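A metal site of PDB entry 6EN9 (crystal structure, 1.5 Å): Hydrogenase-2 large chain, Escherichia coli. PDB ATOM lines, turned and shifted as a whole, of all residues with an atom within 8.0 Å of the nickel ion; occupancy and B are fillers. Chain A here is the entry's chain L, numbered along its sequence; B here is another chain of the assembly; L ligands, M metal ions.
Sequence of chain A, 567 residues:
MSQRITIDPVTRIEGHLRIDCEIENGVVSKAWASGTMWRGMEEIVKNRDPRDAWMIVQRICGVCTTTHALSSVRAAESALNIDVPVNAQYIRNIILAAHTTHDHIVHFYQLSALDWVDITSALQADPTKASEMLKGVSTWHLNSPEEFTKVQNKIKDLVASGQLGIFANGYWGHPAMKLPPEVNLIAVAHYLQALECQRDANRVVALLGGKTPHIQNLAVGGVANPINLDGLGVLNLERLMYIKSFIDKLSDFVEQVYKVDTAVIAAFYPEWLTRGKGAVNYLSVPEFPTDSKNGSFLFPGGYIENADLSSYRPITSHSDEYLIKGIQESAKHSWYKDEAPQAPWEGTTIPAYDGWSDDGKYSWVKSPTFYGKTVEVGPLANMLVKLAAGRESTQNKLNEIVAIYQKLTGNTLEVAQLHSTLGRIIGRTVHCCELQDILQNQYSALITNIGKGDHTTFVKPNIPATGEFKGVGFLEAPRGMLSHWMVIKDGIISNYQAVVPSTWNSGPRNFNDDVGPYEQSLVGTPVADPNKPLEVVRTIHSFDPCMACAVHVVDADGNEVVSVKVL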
ATOM      1  N   GLU A  14       9.711  -3.014   6.456  1.00  0.00           N
ATOM      2  CA  GLU A  14      10.430  -3.642   7.537  1.00  0.00           C
ATOM      3  C   GLU A  14      10.869  -5.045   7.068  1.00  0.00           C
ATOM      4  O   GLU A  14      10.015  -5.864   6.583  1.00  0.00           O
ATOM      5  CB  GLU A  14       9.551  -3.759   8.776  1.00  0.00           C
ATOM      6  CG  GLU A  14      10.251  -4.209  10.042  1.00  0.00           C
ATOM      7  CD  GLU A  14      10.807  -5.643  10.006  1.00  0.00           C
ATOM      8  OE1 GLU A  14      10.101  -6.512   9.435  1.00  0.00           O
ATOM      9  OE2 GLU A  14      11.939  -5.956  10.538  1.00  0.00           O
ATOM     10  N   GLY A  15      12.130  -5.360   7.333  1.00  0.00           N
ATOM     11  CA  GLY A  15      12.627  -6.722   7.138  1.00  0.00           C
ATOM     12  C   GLY A  15      13.072  -7.109   5.779  1.00  0.00           C
ATOM     13  O   GLY A  15      13.322  -6.269   4.892  1.00  0.00           O
ATOM     14  N   GLN A  58       7.277  -9.417  21.962  1.00  0.00           N
ATOM     15  CA  GLN A  58       7.241  -8.022  21.476  1.00  0.00           C
ATOM     16  C   GLN A  58       8.353  -7.828  20.441  1.00  0.00           C
ATOM     17  O   GLN A  58       8.183  -7.065  19.493  1.00  0.00           O
ATOM     18  CB  GLN A  58       7.431  -7.035  22.614  1.00  0.00           C
ATOM     19  CG  GLN A  58       7.175  -5.599  22.117  1.00  0.00           C
ATOM     20  CD  GLN A  58       7.023  -4.482  23.124  1.00  0.00           C
ATOM     21  OE1 GLN A  58       6.470  -3.402  22.777  1.00  0.00           O
ATOM     22  NE2 GLN A  58       7.567  -4.684  24.327  1.00  0.00           N
ATOM     23  N   ILE A  60       9.220  -9.690  18.153  1.00  0.00           N
ATOM     24  CA  ILE A  60       8.933 -10.044  16.759  1.00  0.00           C
ATOM     25  C   ILE A  60       9.160  -8.828  15.854  1.00  0.00           C
ATOM     26  O   ILE A  60       9.639  -9.025  14.722  1.00  0.00           O
ATOM     27  CB  ILE A  60       7.541 -10.608  16.624  1.00  0.00           C
ATOM     28  CG1 ILE A  60       7.532 -12.033  17.226  1.00  0.00           C
ATOM     29  CG2 ILE A  60       7.046 -10.591  15.192  1.00  0.00           C
ATOM     30  CD1 ILE A  60       6.174 -12.653  17.314  1.00  0.00           C
ATOM     31  N   CYS A  61       8.776  -7.633  16.312  1.00  0.00           N
ATOM     32  CA  CYS A  61       8.932  -6.435  15.475  1.00  0.00           C
ATOM     33  C   CYS A  61       9.081  -5.158  16.258  1.00  0.00           C
ATOM     34  O   CYS A  61       8.316  -4.956  17.218  1.00  0.00           O
ATOM     35  CB  CYS A  61       7.728  -6.373  14.566  1.00  0.00           C
ATOM     36  SG  CYS A  61       7.844  -5.115  13.247  1.00  0.00           S
ATOM     37  N   GLY A  62       9.995  -4.321  15.814  1.00  0.00           N
ATOM     38  CA  GLY A  62      10.174  -3.004  16.336  1.00  0.00           C
ATOM     39  C   GLY A  62       9.563  -1.870  15.550  1.00  0.00           C
ATOM     40  O   GLY A  62       9.509  -0.782  16.110  1.00  0.00           O
ATOM     41  N   VAL A  63       9.090  -2.132  14.344  1.00  0.00           N
ATOM     42  CA  VAL A  63       8.278  -1.153  13.626  1.00  0.00           C
ATOM     43  C   VAL A  63       6.907  -1.172  14.304  1.00  0.00           C
ATOM     44  O   VAL A  63       6.469  -0.171  14.846  1.00  0.00           O
ATOM     45  CB  VAL A  63       8.256  -1.424  12.136  1.00  0.00           C
ATOM     46  CG1 VAL A  63       7.317  -0.455  11.449  1.00  0.00           C
ATOM     47  CG2 VAL A  63       9.645  -1.281  11.574  1.00  0.00           C
ATOM     48  N   CYS A  64       6.207  -2.311  14.252  1.00  0.00           N
ATOM     49  CA  CYS A  64       4.959  -2.494  15.019  1.00  0.00           C
ATOM     50  C   CYS A  64       5.275  -2.928  16.414  1.00  0.00           C
ATOM     51  O   CYS A  64       4.690  -3.879  16.954  1.00  0.00           O
ATOM     52  CB  CYS A  64       3.943  -3.409  14.313  1.00  0.00           C
ATOM     53  SG  CYS A  64       4.526  -5.103  14.052  1.00  0.00           S
ATOM     54  N   THR A  65       6.151  -2.160  17.051  1.00  0.00           N
ATOM     55  CA  THR A  65       6.314  -2.249  18.470  1.00  0.00           C
ATOM     56  C   THR A  65       4.956  -2.042  19.145  1.00  0.00           C
ATOM     57  O   THR A  65       4.042  -1.520  18.554  1.00  0.00           O
ATOM     58  CB  THR A  65       7.441  -1.409  18.993  1.00  0.00           C
ATOM     59  OG1 THR A  65       7.728  -1.796  20.345  1.00  0.00           O
ATOM     60  CG2 THR A  65       7.133   0.027  18.942  1.00  0.00           C
ATOM     61  N   THR A  67       2.543  -4.031  19.507  1.00  0.00           N
ATOM     62  CA  THR A  67       1.429  -4.859  19.067  1.00  0.00           C
ATOM     63  C   THR A  67       1.506  -6.293  19.534  1.00  0.00           C
ATOM     64  O   THR A  67       0.512  -6.884  19.960  1.00  0.00           O
ATOM     65  CB  THR A  67       1.230  -4.806  17.515  1.00  0.00           C
ATOM     66  OG1 THR A  67       2.323  -5.437  16.859  1.00  0.00           O
ATOM     67  CG2 THR A  67       1.084  -3.395  17.020  1.00  0.00           C
ATOM     68  N   HIS A  68       2.687  -6.893  19.384  1.00  0.00           N
ATOM     69  CA  HIS A  68       2.882  -8.272  19.845  1.00  0.00           C
ATOM     70  C   HIS A  68       2.903  -8.398  21.334  1.00  0.00           C
ATOM     71  O   HIS A  68       2.457  -9.440  21.878  1.00  0.00           O
ATOM     72  CB  HIS A  68       4.144  -8.869  19.239  1.00  0.00           C
ATOM     73  CG  HIS A  68       4.078  -9.001  17.768  1.00  0.00           C
ATOM     74  ND1 HIS A  68       3.383 -10.013  17.135  1.00  0.00           N
ATOM     75  CD2 HIS A  68       4.561  -8.197  16.798  1.00  0.00           C
ATOM     76  CE1 HIS A  68       3.505  -9.842  15.822  1.00  0.00           C
ATOM     77  NE2 HIS A  68       4.174  -8.727  15.589  1.00  0.00           N
ATOM     78  N   HIS A  99       0.869   4.727  18.972  1.00  0.00           N
ATOM     79  CA  HIS A  99       1.829   3.986  18.179  1.00  0.00           C
ATOM     80  C   HIS A  99       1.423   3.941  16.702  1.00  0.00           C
ATOM     81  O   HIS A  99       2.236   4.200  15.787  1.00  0.00           O
ATOM     82  CB  HIS A  99       2.009   2.520  18.659  1.00  0.00           C
ATOM     83  CG  HIS A  99       2.821   1.781  17.662  1.00  0.00           C
ATOM     84  ND1 HIS A  99       4.180   1.970  17.599  1.00  0.00           N
ATOM     85  CD2 HIS A  99       2.478   1.083  16.557  1.00  0.00           C
ATOM     86  CE1 HIS A  99       4.632   1.356  16.513  1.00  0.00           C
ATOM     87  NE2 HIS A  99       3.625   0.798  15.881  1.00  0.00           N
ATOM     88  N   ASP A 103       3.160   4.996  13.195  1.00  0.00           N
ATOM     89  CA  ASP A 103       3.507   3.950  12.270  1.00  0.00           C
ATOM     90  C   ASP A 103       2.963   4.354  10.878  1.00  0.00           C
ATOM     91  O   ASP A 103       3.703   4.332   9.880  1.00  0.00           O
ATOM     92  CB  ASP A 103       2.945   2.620  12.865  1.00  0.00           C
ATOM     93  CG  ASP A 103       3.495   1.391  12.246  1.00  0.00           C
ATOM     94  OD1 ASP A 103       3.849   1.411  11.040  1.00  0.00           O
ATOM     95  OD2 ASP A 103       3.475   0.339  12.968  1.00  0.00           O
ATOM     96  N   ALA A 477      -3.881  -4.508  14.356  1.00  0.00           N
ATOM     97  CA  ALA A 477      -2.561  -3.855  14.296  1.00  0.00           C
ATOM     98  C   ALA A 477      -2.516  -2.913  13.094  1.00  0.00           C
ATOM     99  O   ALA A 477      -3.429  -2.941  12.235  1.00  0.00           O
ATOM    100  CB  ALA A 477      -1.467  -4.940  14.206  1.00  0.00           C
ATOM    101  N   PRO A 478      -1.458  -2.129  12.990  1.00  0.00           N
ATOM    102  CA  PRO A 478      -1.391  -1.182  11.862  1.00  0.00           C
ATOM    103  C   PRO A 478      -1.485  -1.852  10.517  1.00  0.00           C
ATOM    104  O   PRO A 478      -2.012  -1.282   9.592  1.00  0.00           O
ATOM    105  CB  PRO A 478      -0.016  -0.520  12.053  1.00  0.00           C
ATOM    106  CG  PRO A 478       0.227  -0.558  13.546  1.00  0.00           C
ATOM    107  CD  PRO A 478      -0.431  -1.831  14.025  1.00  0.00           C
ATOM    108  N   ARG A 479      -1.027  -3.101  10.413  1.00  0.00           N
ATOM    109  CA  ARG A 479      -1.014  -3.841   9.183  1.00  0.00           C
ATOM    110  C   ARG A 479      -2.138  -4.822   9.055  1.00  0.00           C
ATOM    111  O   ARG A 479      -2.222  -5.543   8.065  1.00  0.00           O
ATOM    112  CB  ARG A 479       0.341  -4.501   8.956  1.00  0.00           C
ATOM    113  CG  ARG A 479       1.431  -3.483   8.715  1.00  0.00           C
ATOM    114  CD  ARG A 479       2.904  -3.958   8.915  1.00  0.00           C
ATOM    115  NE  ARG A 479       3.788  -2.810   8.779  1.00  0.00           N
ATOM    116  CZ  ARG A 479       3.948  -1.842   9.676  1.00  0.00           C
ATOM    117  NH1 ARG A 479       3.466  -1.925  10.885  1.00  0.00           N
ATOM    118  NH2 ARG A 479       4.615  -0.751   9.359  1.00  0.00           N
ATOM    119  N   VAL A 500       0.259 -13.405  11.915  1.00  0.00           N
ATOM    120  CA  VAL A 500       0.517 -11.977  11.919  1.00  0.00           C
ATOM    121  C   VAL A 500      -0.050 -11.368  10.641  1.00  0.00           C
ATOM    122  O   VAL A 500      -0.164 -12.052   9.639  1.00  0.00           O
ATOM    123  CB  VAL A 500       2.040 -11.738  12.107  1.00  0.00           C
ATOM    124  CG1 VAL A 500       2.430 -10.301  12.303  1.00  0.00           C
ATOM    125  CG2 VAL A 500       2.557 -12.536  13.311  1.00  0.00           C
ATOM    126  N   PRO A 501      -0.427 -10.089  10.643  1.00  0.00           N
ATOM    127  CA  PRO A 501      -1.092  -9.581   9.447  1.00  0.00           C
ATOM    128  C   PRO A 501      -0.292  -9.715   8.153  1.00  0.00           C
ATOM    129  O   PRO A 501      -0.838 -10.176   7.142  1.00  0.00           O
ATOM    130  CB  PRO A 501      -1.470  -8.131   9.794  1.00  0.00           C
ATOM    131  CG  PRO A 501      -0.751  -7.844  11.053  1.00  0.00           C
ATOM    132  CD  PRO A 501      -0.594  -9.164  11.760  1.00  0.00           C
ATOM    133  N   SER A 502       0.993  -9.397   8.180  1.00  0.00           N
ATOM    134  CA  SER A 502       1.774  -9.571   6.943  1.00  0.00           C
ATOM    135  C   SER A 502       1.942 -11.056   6.588  1.00  0.00           C
ATOM    136  O   SER A 502       2.262 -11.345   5.449  1.00  0.00           O
ATOM    137  CB  SER A 502       3.131  -8.904   7.078  1.00  0.00           C
ATOM    138  OG  SER A 502       2.988  -7.503   7.105  1.00  0.00           O
ATOM    139  N   ASP A 544       2.251  -2.252   3.193  1.00  0.00           N
ATOM    140  CA  ASP A 544       3.089  -1.969   4.359  1.00  0.00           C
ATOM    141  C   ASP A 544       3.746  -3.264   4.882  1.00  0.00           C
ATOM    142  O   ASP A 544       3.538  -3.663   6.027  1.00  0.00           O
ATOM    143  CB  ASP A 544       2.197  -1.242   5.366  1.00  0.00           C
ATOM    144  CG  ASP A 544       2.909  -0.684   6.545  1.00  0.00           C
ATOM    145  OD1 ASP A 544       4.177  -0.688   6.622  1.00  0.00           O
ATOM    146  OD2 ASP A 544       2.140  -0.255   7.484  1.00  0.00           O
ATOM    147  N   PRO A 545       4.513  -3.939   4.007  1.00  0.00           N
ATOM    148  CA  PRO A 545       5.110  -5.179   4.464  1.00  0.00           C
ATOM    149  C   PRO A 545       5.976  -5.062   5.716  1.00  0.00           C
ATOM    150  O   PRO A 545       6.798  -4.143   5.866  1.00  0.00           O
ATOM    151  CB  PRO A 545       5.966  -5.636   3.282  1.00  0.00           C
ATOM    152  CG  PRO A 545       5.377  -4.892   2.092  1.00  0.00           C
ATOM    153  CD  PRO A 545       4.974  -3.566   2.645  1.00  0.00           C
ATOM    154  N   CYS A 546       5.792  -6.095   6.467  1.00  0.00           N
ATOM    155  CA  CYS A 546       6.651  -6.175   7.649  1.00  0.00           C
ATOM    156  C   CYS A 546       7.080  -7.630   7.742  1.00  0.00           C
ATOM    157  O   CYS A 546       6.276  -8.483   8.127  1.00  0.00           O
ATOM    158  CB  CYS A 546       5.918  -5.730   8.917  1.00  0.00           C
ATOM    159  SG  CYS A 546       6.944  -5.718  10.409  1.00  0.00           S
ATOM    160  N   MET A 547       8.316  -7.970   7.400  1.00  0.00           N
ATOM    161  CA  MET A 547       8.727  -9.380   7.283  1.00  0.00           C
ATOM    162  C   MET A 547       9.213 -10.046   8.549  1.00  0.00           C
ATOM    163  O   MET A 547       9.098 -11.268   8.686  1.00  0.00           O
ATOM    164  CB  MET A 547       9.712  -9.586   6.149  1.00  0.00           C
ATOM    165  CG  MET A 547       9.182  -9.027   4.832  1.00  0.00           C
ATOM    166  SD  MET A 547       7.542  -9.483   4.311  1.00  0.00           S
ATOM    167  CE  MET A 547       7.800 -11.270   4.084  1.00  0.00           C
ATOM    168  N   ALA A 548       9.704  -9.242   9.490  1.00  0.00           N
ATOM    169  CA  ALA A 548       9.975  -9.753  10.844  1.00  0.00           C
ATOM    170  C   ALA A 548       8.643 -10.224  11.421  1.00  0.00           C
ATOM    171  O   ALA A 548       8.509 -11.327  11.991  1.00  0.00           O
ATOM    172  CB  ALA A 548      10.636  -8.678  11.700  1.00  0.00           C
ATOM    173  N   CYS A 549       7.601  -9.425  11.216  1.00  0.00           N
ATOM    174  CA  CYS A 549       6.224  -9.856  11.525  1.00  0.00           C
ATOM    175  C   CYS A 549       5.773 -11.060  10.749  1.00  0.00           C
ATOM    176  O   CYS A 549       5.231 -12.006  11.328  1.00  0.00           O
ATOM    177  CB  CYS A 549       5.236  -8.731  11.258  1.00  0.00           C
ATOM    178  SG  CYS A 549       5.048  -7.636  12.688  1.00  0.00           S
ATOM    179  N   ALA A 550       5.953 -11.056   9.416  1.00  0.00           N
ATOM    180  CA  ALA A 550       5.353 -12.113   8.629  1.00  0.00           C
ATOM    181  C   ALA A 550       5.896 -13.470   9.032  1.00  0.00           C
ATOM    182  O   ALA A 550       5.156 -14.449   8.987  1.00  0.00           O
ATOM    183  CB  ALA A 550       5.616 -11.882   7.146  1.00  0.00           C
ATOM    184  N   CYS B  21      14.738  -6.876  14.318  1.00  0.00           N
ATOM    185  CA  CYS B  21      13.313  -6.596  14.360  1.00  0.00           C
ATOM    186  C   CYS B  21      13.029  -5.201  13.855  1.00  0.00           C
ATOM    187  O   CYS B  21      11.881  -4.815  13.785  1.00  0.00           O
ATOM    188  CB  CYS B  21      12.742  -6.761  15.794  1.00  0.00           C
ATOM    189  SG  CYS B  21      13.104  -5.355  16.882  1.00  0.00           S
ATOM    190  N   THR B  22      14.068  -4.382  13.639  1.00  0.00           N
ATOM    191  CA  THR B  22      14.013  -2.979  13.127  1.00  0.00           C
ATOM    192  C   THR B  22      13.840  -1.959  14.267  1.00  0.00           C
ATOM    193  O   THR B  22      13.963  -0.778  14.068  1.00  0.00           O
ATOM    194  CB  THR B  22      13.035  -2.781  11.952  1.00  0.00           C
ATOM    195  OG1 THR B  22      13.292  -3.886  11.017  1.00  0.00           O
ATOM    196  CG2 THR B  22      13.199  -1.456  11.263  1.00  0.00           C
HETATM  197 FE1  LIG L   1       3.322  -6.159  12.463  1.00  0.00          FE
HETATM  198  C1  LIG L   1       2.802  -6.923  10.860  1.00  0.00           C
HETATM  199  N1  LIG L   1       2.513  -7.372   9.833  1.00  0.00           N
HETATM  200  C2  LIG L   1       2.105  -4.804  12.268  1.00  0.00           C
HETATM  201  N2  LIG L   1       1.354  -3.944  12.111  1.00  0.00           N
HETATM  202  C3  LIG L   1       2.051  -6.997  13.463  1.00  0.00           C
HETATM  203  O1  LIG L   1       1.230  -7.476  14.052  1.00  0.00           O
HETATM  204 NI    NI M   1       5.888  -5.469  12.256  1.00  0.00          NI
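The side-chain sulfur (SG) of Cys 549 binds an iron atom (FE1) of the ligand, at 2.3 Å.
A nitrogen (N2) of the ligand is in hydrogen-bond range of the guanidinium group (NH1) of Arg 479, 3.2 Å away.
OG of Ser 502 sits at hydrogen-bond distance from N1 of the ligand (2.8 Å).
The backbone NH of Arg 479 lies within hydrogen-bond range of a nitrogen (N2) of the ligand.
An iron atom (FE1) of the ligand is bound by the side-chain sulfur (SG) of Cys 64 (2.3 Å).
The backbone NH (N) of Ser 502 lies within hydrogen-bond range of a nitrogen (N1) of the ligand, 3.0 Å away.
The backbone carbonyl oxygen of Cys 64 is in hydrogen-bond range of the side-chain hydroxyl of Thr 67.
The backbone NH (N) of Cys 546 is in hydrogen-bond range of the side-chain hydroxyl (OG) of Ser 502, 3.2 Å away.
The side-chain sulfur of Cys 549 sits close to a ring nitrogen (NE2) of His 68, 3.2 Å away.
The side-chain carboxylate (OE1) of Glu 14 sits close to the side-chain sulfur (SG) of Cys 546.
N of Val 63 sits close to SG of Cys 61, 3.4 Å away.
Of the 28 residues printed, 4 come within 4 Å of the nickel ion.
The nearest printed residue that does not touch the nickel ion is Arg 479 (4.5 Å).
The nickel ion is bound by the side-chain sulfur of Cys 546 (2.1 Å), the side-chain sulfur of Cys 61 (2.2 Å), the side-chain sulfur of Cys 64 (2.3 Å) and the side-chain sulfur of Cys 549 (2.4 Å).
The nickel ion has four donor atoms within binding distance.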
